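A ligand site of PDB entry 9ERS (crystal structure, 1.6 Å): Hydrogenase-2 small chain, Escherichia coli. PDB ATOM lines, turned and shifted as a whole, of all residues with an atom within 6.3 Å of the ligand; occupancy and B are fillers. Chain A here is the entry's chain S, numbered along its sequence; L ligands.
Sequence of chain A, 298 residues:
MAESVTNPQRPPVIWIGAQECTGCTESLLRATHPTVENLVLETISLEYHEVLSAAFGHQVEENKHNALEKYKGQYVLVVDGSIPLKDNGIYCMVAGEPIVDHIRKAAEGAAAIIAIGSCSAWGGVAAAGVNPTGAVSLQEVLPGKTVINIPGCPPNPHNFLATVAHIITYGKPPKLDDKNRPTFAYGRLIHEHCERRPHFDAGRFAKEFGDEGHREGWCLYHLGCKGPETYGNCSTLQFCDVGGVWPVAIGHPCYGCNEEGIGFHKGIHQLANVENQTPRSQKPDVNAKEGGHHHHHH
The backbone NH (N) of Cys 225 sits at hydrogen-bond distance from the backbone carbonyl oxygen (O) of Leu 220 (3.3 Å).
The backbone NH (N) of Arg 196 lies close to the side-chain sulfur (SG) of Cys 194, 3.4 Å away.
N of Tyr 221 sits close to SG of Cys 219.
The guanidinium group (NH1) of Arg 196 lies within hydrogen-bond range of the backbone carbonyl oxygen (O) of Trp 218 (2.9 Å).
The backbone NH of His 191 lies within hydrogen-bond range of the backbone carbonyl oxygen of Gly 227 (3.2 Å).
The side-chain sulfur (SG) of Cys 225 sits close to the backbone NH (N) of Cys 254 (3.6 Å).
OE1 of Glu 192 lies within salt-bridge range of NH1 of Arg 197, at 3.1 Å.
N of Gly 227 lies close to SG of Cys 225, at 3.5 Å.
The backbone carbonyl oxygen of Arg 196 lies close to a sulfur (S2) of the ligand, 3.7 Å away.
Residues that only touch the ligand: Tyr 221, Gly 227, Val 248 and Phe 200.
Hydrophobic or aromatic side chains that line the ligand: His 191, Phe 200, Tyr 221 and Val 248.
Within 4 Å of the ligand: His 191, Cys 194, Arg 196, Arg 197, Phe 200, Cys 219, Leu 220, Tyr 221, Cys 225, Gly 227 and Val 248.
The nearest printed residue that does not touch the ligand is Pro 228 (4.01 Å).
ND1 of His 191 is bound to FE3 of the ligand, 2.0 Å away.
FE1 of the ligand is bound by SG of Cys 219 (2.3 Å).
An iron atom (FE2) of the ligand is bound by the side-chain sulfur (SG) of Cys 225.
N of Arg 197 sits close to S2 of the ligand, 3.4 Å away.
The side-chain sulfur of Cys 194 binds an iron atom (FE4) of the ligand (2.3 Å).
A sulfur (S3) of the ligand sits close to the backbone NH (N) of Leu 220.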
ATOM      1  N   ILE A 190       8.907  10.571  -4.375  1.00  0.00           N
ATOM      2  CA  ILE A 190       9.730  11.057  -5.467  1.00  0.00           C
ATOM      3  C   ILE A 190       9.001  12.219  -6.178  1.00  0.00           C
ATOM      4  O   ILE A 190       9.624  13.221  -6.513  1.00  0.00           O
ATOM      5  CB  ILE A 190      10.112   9.890  -6.397  1.00  0.00           C
ATOM      6  CG1 ILE A 190      11.120   8.959  -5.712  1.00  0.00           C
ATOM      7  CG2 ILE A 190      10.660  10.424  -7.711  1.00  0.00           C
ATOM      8  CD1 ILE A 190      11.372   7.659  -6.449  1.00  0.00           C
ATOM      9  N   HIS A 191       7.681  12.072  -6.376  1.00  0.00           N
ATOM     10  CA  HIS A 191       6.896  13.050  -7.122  1.00  0.00           C
ATOM     11  C   HIS A 191       6.714  14.348  -6.315  1.00  0.00           C
ATOM     12  O   HIS A 191       6.344  15.373  -6.891  1.00  0.00           O
ATOM     13  CB  HIS A 191       5.537  12.438  -7.458  1.00  0.00           C
ATOM     14  CG  HIS A 191       4.577  13.298  -8.151  1.00  0.00           C
ATOM     15  ND1 HIS A 191       4.595  13.505  -9.517  1.00  0.00           N
ATOM     16  CD2 HIS A 191       3.484  13.929  -7.678  1.00  0.00           C
ATOM     17  CE1 HIS A 191       3.552  14.268  -9.847  1.00  0.00           C
ATOM     18  NE2 HIS A 191       2.877  14.549  -8.735  1.00  0.00           N
ATOM     19  N   GLU A 192       6.972  14.301  -5.003  1.00  0.00           N
ATOM     20  CA  GLU A 192       6.900  15.487  -4.173  1.00  0.00           C
ATOM     21  C   GLU A 192       8.276  16.131  -4.047  1.00  0.00           C
ATOM     22  O   GLU A 192       8.471  17.061  -3.241  1.00  0.00           O
ATOM     23  CB  GLU A 192       6.291  15.170  -2.805  1.00  0.00           C
ATOM     24  CG  GLU A 192       4.807  14.813  -2.867  1.00  0.00           C
ATOM     25  CD  GLU A 192       3.924  15.864  -3.525  1.00  0.00           C
ATOM     26  OE1 GLU A 192       3.225  15.536  -4.498  1.00  0.00           O
ATOM     27  OE2 GLU A 192       3.952  17.031  -3.085  1.00  0.00           O
ATOM     28  N   CYS A 194      10.361  16.062  -7.404  1.00  0.00           N
ATOM     29  CA  CYS A 194      10.827  15.745  -8.746  1.00  0.00           C
ATOM     30  C   CYS A 194      10.890  16.994  -9.618  1.00  0.00           C
ATOM     31  O   CYS A 194       9.933  17.789  -9.669  1.00  0.00           O
ATOM     32  CB  CYS A 194       9.879  14.770  -9.413  1.00  0.00           C
ATOM     33  SG  CYS A 194      10.315  14.388 -11.133  1.00  0.00           S
ATOM     34  N   GLU A 195      12.023  17.145 -10.331  1.00  0.00           N
ATOM     35  CA  GLU A 195      12.300  18.345 -11.121  1.00  0.00           C
ATOM     36  C   GLU A 195      11.387  18.429 -12.345  1.00  0.00           C
ATOM     37  O   GLU A 195      11.396  19.459 -13.031  1.00  0.00           O
ATOM     38  CB  GLU A 195      13.781  18.406 -11.511  1.00  0.00           C
ATOM     39  CG  GLU A 195      14.262  17.331 -12.484  1.00  0.00           C
ATOM     40  CD  GLU A 195      14.702  15.987 -11.909  1.00  0.00           C
ATOM     41  OE1 GLU A 195      14.397  15.709 -10.712  1.00  0.00           O
ATOM     42  OE2 GLU A 195      15.330  15.205 -12.668  1.00  0.00           O
ATOM     43  N   ARG A 196      10.614  17.368 -12.649  1.00  0.00           N
ATOM     44  CA  ARG A 196       9.695  17.426 -13.772  1.00  0.00           C
ATOM     45  C   ARG A 196       8.272  17.773 -13.312  1.00  0.00           C
ATOM     46  O   ARG A 196       7.358  17.868 -14.116  1.00  0.00           O
ATOM     47  CB  ARG A 196       9.748  16.142 -14.589  1.00  0.00           C
ATOM     48  CG  ARG A 196      11.150  15.848 -15.090  1.00  0.00           C
ATOM     49  CD  ARG A 196      11.166  14.839 -16.205  1.00  0.00           C
ATOM     50  NE  ARG A 196      12.523  14.678 -16.660  1.00  0.00           N
ATOM     51  CZ  ARG A 196      12.879  14.112 -17.805  1.00  0.00           C
ATOM     52  NH1 ARG A 196      11.972  13.554 -18.582  1.00  0.00           N
ATOM     53  NH2 ARG A 196      14.148  14.082 -18.153  1.00  0.00           N
ATOM     54  N   ARG A 197       8.094  18.054 -12.029  1.00  0.00           N
ATOM     55  CA  ARG A 197       6.805  18.458 -11.521  1.00  0.00           C
ATOM     56  C   ARG A 197       6.213  19.643 -12.302  1.00  0.00           C
ATOM     57  O   ARG A 197       5.009  19.675 -12.554  1.00  0.00           O
ATOM     58  CB  ARG A 197       6.889  18.785 -10.038  1.00  0.00           C
ATOM     59  CG  ARG A 197       5.541  19.152  -9.439  1.00  0.00           C
ATOM     60  CD  ARG A 197       4.471  18.089  -9.673  1.00  0.00           C
ATOM     61  NE  ARG A 197       3.274  18.400  -8.922  1.00  0.00           N
ATOM     62  CZ  ARG A 197       3.094  18.141  -7.646  1.00  0.00           C
ATOM     63  NH1 ARG A 197       3.800  17.226  -7.011  1.00  0.00           N
ATOM     64  NH2 ARG A 197       2.109  18.755  -7.002  1.00  0.00           N
ATOM     65  N   PRO A 198       7.004  20.672 -12.707  1.00  0.00           N
ATOM     66  CA  PRO A 198       6.419  21.784 -13.466  1.00  0.00           C
ATOM     67  C   PRO A 198       5.715  21.317 -14.746  1.00  0.00           C
ATOM     68  O   PRO A 198       4.698  21.891 -15.132  1.00  0.00           O
ATOM     69  CB  PRO A 198       7.639  22.661 -13.797  1.00  0.00           C
ATOM     70  CG  PRO A 198       8.621  22.347 -12.688  1.00  0.00           C
ATOM     71  CD  PRO A 198       8.426  20.873 -12.400  1.00  0.00           C
ATOM     72  N   PHE A 200       4.470  18.222 -15.299  1.00  0.00           N
ATOM     73  CA  PHE A 200       3.252  17.573 -14.823  1.00  0.00           C
ATOM     74  C   PHE A 200       2.172  18.632 -14.631  1.00  0.00           C
ATOM     75  O   PHE A 200       1.046  18.480 -15.109  1.00  0.00           O
ATOM     76  CB  PHE A 200       3.545  16.805 -13.533  1.00  0.00           C
ATOM     77  CG  PHE A 200       2.358  16.113 -12.907  1.00  0.00           C
ATOM     78  CD1 PHE A 200       1.523  16.775 -12.024  1.00  0.00           C
ATOM     79  CD2 PHE A 200       2.101  14.770 -13.163  1.00  0.00           C
ATOM     80  CE1 PHE A 200       0.456  16.120 -11.419  1.00  0.00           C
ATOM     81  CE2 PHE A 200       1.024  14.117 -12.567  1.00  0.00           C
ATOM     82  CZ  PHE A 200       0.203  14.797 -11.695  1.00  0.00           C
ATOM     83  N   PHE A 205       3.545  16.408 -21.205  1.00  0.00           N
ATOM     84  CA  PHE A 205       3.790  14.991 -20.989  1.00  0.00           C
ATOM     85  C   PHE A 205       4.402  14.322 -22.212  1.00  0.00           C
ATOM     86  O   PHE A 205       3.937  14.516 -23.328  1.00  0.00           O
ATOM     87  CB  PHE A 205       2.491  14.231 -20.661  1.00  0.00           C
ATOM     88  CG  PHE A 205       1.777  14.635 -19.392  1.00  0.00           C
ATOM     89  CD1 PHE A 205       2.356  14.402 -18.155  1.00  0.00           C
ATOM     90  CD2 PHE A 205       0.527  15.232 -19.428  1.00  0.00           C
ATOM     91  CE1 PHE A 205       1.691  14.743 -16.994  1.00  0.00           C
ATOM     92  CE2 PHE A 205      -0.126  15.581 -18.258  1.00  0.00           C
ATOM     93  CZ  PHE A 205       0.452  15.337 -17.040  1.00  0.00           C
ATOM     94  N   TRP A 218      10.113  16.417 -20.678  1.00  0.00           N
ATOM     95  CA  TRP A 218       8.824  16.570 -20.023  1.00  0.00           C
ATOM     96  C   TRP A 218       8.547  15.426 -19.044  1.00  0.00           C
ATOM     97  O   TRP A 218       9.273  14.442 -18.968  1.00  0.00           O
ATOM     98  CB  TRP A 218       7.732  16.683 -21.098  1.00  0.00           C
ATOM     99  CG  TRP A 218       7.761  17.972 -21.861  1.00  0.00           C
ATOM    100  CD1 TRP A 218       8.662  19.003 -21.736  1.00  0.00           C
ATOM    101  CD2 TRP A 218       6.852  18.397 -22.893  1.00  0.00           C
ATOM    102  NE1 TRP A 218       8.374  20.015 -22.602  1.00  0.00           N
ATOM    103  CE2 TRP A 218       7.263  19.671 -23.335  1.00  0.00           C
ATOM    104  CE3 TRP A 218       5.715  17.816 -23.489  1.00  0.00           C
ATOM    105  CZ2 TRP A 218       6.582  20.389 -24.324  1.00  0.00           C
ATOM    106  CZ3 TRP A 218       5.052  18.521 -24.458  1.00  0.00           C
ATOM    107  CH2 TRP A 218       5.471  19.785 -24.870  1.00  0.00           C
ATOM    108  N   CYS A 219       7.451  15.575 -18.289  1.00  0.00           N
ATOM    109  CA  CYS A 219       7.046  14.619 -17.285  1.00  0.00           C
ATOM    110  C   CYS A 219       6.727  13.258 -17.931  1.00  0.00           C
ATOM    111  O   CYS A 219       6.265  13.207 -19.060  1.00  0.00           O
ATOM    112  CB  CYS A 219       5.844  15.165 -16.540  1.00  0.00           C
ATOM    113  SG  CYS A 219       5.031  13.995 -15.430  1.00  0.00           S
ATOM    114  N   LEU A 220       7.014  12.182 -17.213  1.00  0.00           N
ATOM    115  CA  LEU A 220       6.867  10.823 -17.688  1.00  0.00           C
ATOM    116  C   LEU A 220       5.649  10.126 -17.072  1.00  0.00           C
ATOM    117  O   LEU A 220       5.507   8.907 -17.211  1.00  0.00           O
ATOM    118  CB  LEU A 220       8.156  10.073 -17.348  1.00  0.00           C
ATOM    119  CG  LEU A 220       9.472  10.703 -17.842  1.00  0.00           C
ATOM    120  CD1 LEU A 220      10.630   9.741 -17.637  1.00  0.00           C
ATOM    121  CD2 LEU A 220       9.373  11.093 -19.293  1.00  0.00           C
ATOM    122  N   TYR A 221       4.731  10.879 -16.452  1.00  0.00           N
ATOM    123  CA  TYR A 221       3.550  10.318 -15.829  1.00  0.00           C
ATOM    124  C   TYR A 221       2.814   9.376 -16.796  1.00  0.00           C
ATOM    125  O   TYR A 221       2.472   8.250 -16.408  1.00  0.00           O
ATOM    126  CB  TYR A 221       2.583  11.393 -15.327  1.00  0.00           C
ATOM    127  CG  TYR A 221       1.361  10.778 -14.723  1.00  0.00           C
ATOM    128  CD1 TYR A 221       1.413  10.189 -13.477  1.00  0.00           C
ATOM    129  CD2 TYR A 221       0.196  10.628 -15.471  1.00  0.00           C
ATOM    130  CE1 TYR A 221       0.326   9.536 -12.932  1.00  0.00           C
ATOM    131  CE2 TYR A 221      -0.910   9.978 -14.955  1.00  0.00           C
ATOM    132  CZ  TYR A 221      -0.823   9.413 -13.690  1.00  0.00           C
ATOM    133  OH  TYR A 221      -1.892   8.746 -13.174  1.00  0.00           O
ATOM    134  N   HIS A 222       2.602   9.823 -18.048  1.00  0.00           N
ATOM    135  CA  HIS A 222       1.797   9.049 -18.980  1.00  0.00           C
ATOM    136  C   HIS A 222       2.603   7.929 -19.630  1.00  0.00           C
ATOM    137  O   HIS A 222       2.034   7.223 -20.463  1.00  0.00           O
ATOM    138  CB  HIS A 222       1.090   9.943 -20.024  1.00  0.00           C
ATOM    139  CG  HIS A 222      -0.100  10.605 -19.442  1.00  0.00           C
ATOM    140  ND1 HIS A 222      -1.264   9.908 -19.245  1.00  0.00           N
ATOM    141  CD2 HIS A 222      -0.311  11.850 -18.963  1.00  0.00           C
ATOM    142  CE1 HIS A 222      -2.133  10.702 -18.626  1.00  0.00           C
ATOM    143  NE2 HIS A 222      -1.577  11.903 -18.456  1.00  0.00           N
ATOM    144  N   CYS A 225       5.095   6.578 -14.972  1.00  0.00           N
ATOM    145  CA  CYS A 225       5.960   6.928 -13.859  1.00  0.00           C
ATOM    146  C   CYS A 225       5.258   6.659 -12.523  1.00  0.00           C
ATOM    147  O   CYS A 225       4.155   7.121 -12.316  1.00  0.00           O
ATOM    148  CB  CYS A 225       6.403   8.378 -13.956  1.00  0.00           C
ATOM    149  SG  CYS A 225       7.656   8.789 -12.714  1.00  0.00           S
ATOM    150  N   LYS A 226       5.956   5.977 -11.604  1.00  0.00           N
ATOM    151  CA  LYS A 226       5.418   5.604 -10.305  1.00  0.00           C
ATOM    152  C   LYS A 226       5.897   6.538  -9.208  1.00  0.00           C
ATOM    153  O   LYS A 226       5.641   6.301  -8.022  1.00  0.00           O
ATOM    154  CB  LYS A 226       5.812   4.171  -9.968  1.00  0.00           C
ATOM    155  CG  LYS A 226       5.330   3.119 -10.962  1.00  0.00           C
ATOM    156  CD  LYS A 226       3.874   3.268 -11.328  1.00  0.00           C
ATOM    157  CE  LYS A 226       3.324   2.131 -12.160  1.00  0.00           C
ATOM    158  NZ  LYS A 226       4.078   1.933 -13.424  1.00  0.00           N
ATOM    159  N   GLY A 227       6.588   7.627  -9.595  1.00  0.00           N
ATOM    160  CA  GLY A 227       7.040   8.624  -8.639  1.00  0.00           C
ATOM    161  C   GLY A 227       5.916   9.058  -7.681  1.00  0.00           C
ATOM    162  O   GLY A 227       6.162   9.265  -6.476  1.00  0.00           O
ATOM    163  N   PRO A 228       4.666   9.216  -8.157  1.00  0.00           N
ATOM    164  CA  PRO A 228       3.568   9.624  -7.268  1.00  0.00           C
ATOM    165  C   PRO A 228       3.232   8.657  -6.144  1.00  0.00           C
ATOM    166  O   PRO A 228       2.562   9.065  -5.195  1.00  0.00           O
ATOM    167  CB  PRO A 228       2.387   9.807  -8.225  1.00  0.00           C
ATOM    168  CG  PRO A 228       3.031  10.098  -9.542  1.00  0.00           C
ATOM    169  CD  PRO A 228       4.255   9.209  -9.568  1.00  0.00           C
ATOM    170  N   TRP A 246      19.445   9.610 -12.741  1.00  0.00           N
ATOM    171  CA  TRP A 246      18.429   8.740 -12.190  1.00  0.00           C
ATOM    172  C   TRP A 246      17.484   8.344 -13.322  1.00  0.00           C
ATOM    173  O   TRP A 246      17.579   8.909 -14.426  1.00  0.00           O
ATOM    174  CB  TRP A 246      17.688   9.371 -11.017  1.00  0.00           C
ATOM    175  CG  TRP A 246      16.749  10.514 -11.277  1.00  0.00           C
ATOM    176  CD1 TRP A 246      17.047  11.781 -11.689  1.00  0.00           C
ATOM    177  CD2 TRP A 246      15.335  10.529 -10.979  1.00  0.00           C
ATOM    178  NE1 TRP A 246      15.939  12.586 -11.661  1.00  0.00           N
ATOM    179  CE2 TRP A 246      14.853  11.828 -11.263  1.00  0.00           C
ATOM    180  CE3 TRP A 246      14.423   9.566 -10.515  1.00  0.00           C
ATOM    181  CZ2 TRP A 246      13.515  12.181 -11.103  1.00  0.00           C
ATOM    182  CZ3 TRP A 246      13.102   9.906 -10.365  1.00  0.00           C
ATOM    183  CH2 TRP A 246      12.654  11.219 -10.619  1.00  0.00           C
ATOM    184  N   VAL A 248      14.360   8.748 -14.336  1.00  0.00           N
ATOM    185  CA  VAL A 248      13.555   9.784 -14.973  1.00  0.00           C
ATOM    186  C   VAL A 248      14.451  10.763 -15.737  1.00  0.00           C
ATOM    187  O   VAL A 248      14.158  11.107 -16.867  1.00  0.00           O
ATOM    188  CB  VAL A 248      12.641  10.465 -13.941  1.00  0.00           C
ATOM    189  CG1 VAL A 248      12.054  11.788 -14.466  1.00  0.00           C
ATOM    190  CG2 VAL A 248      11.520   9.520 -13.529  1.00  0.00           C
ATOM    191  N   PRO A 253      10.408   6.236 -16.957  1.00  0.00           N
ATOM    192  CA  PRO A 253       9.598   6.351 -15.751  1.00  0.00           C
ATOM    193  C   PRO A 253      10.191   5.553 -14.580  1.00  0.00           C
ATOM    194  O   PRO A 253      10.872   4.541 -14.763  1.00  0.00           O
ATOM    195  CB  PRO A 253       8.214   5.813 -16.159  1.00  0.00           C
ATOM    196  CG  PRO A 253       8.463   5.011 -17.389  1.00  0.00           C
ATOM    197  CD  PRO A 253       9.625   5.676 -18.074  1.00  0.00           C
ATOM    198  N   CYS A 254       9.960   6.086 -13.383  1.00  0.00           N
ATOM    199  CA  CYS A 254      10.102   5.326 -12.163  1.00  0.00           C
ATOM    200  C   CYS A 254       9.159   4.130 -12.264  1.00  0.00           C
ATOM    201  O   CYS A 254       8.050   4.279 -12.809  1.00  0.00           O
ATOM    202  CB  CYS A 254       9.802   6.188 -10.955  1.00  0.00           C
ATOM    203  SG  CYS A 254       9.777   5.316  -9.372  1.00  0.00           S
HETATM  204 FE1  LIG L   1       6.272  13.414 -13.624  1.00  0.00          FE
HETATM  205 FE2  LIG L   1       7.238  11.067 -12.442  1.00  0.00          FE
HETATM  206 FE3  LIG L   1       5.910  12.939 -10.971  1.00  0.00          FE
HETATM  207 FE4  LIG L   1       8.398  13.454 -11.922  1.00  0.00          FE
HETATM  208  S1  LIG L   1       7.810  11.773 -10.379  1.00  0.00           S
HETATM  209  S2  LIG L   1       6.617  14.937 -11.981  1.00  0.00           S
HETATM  210  S3  LIG L   1       8.344  12.477 -13.918  1.00  0.00           S
HETATM  211  S4  LIG L   1       5.010  11.706 -12.641  1.00  0.00           S
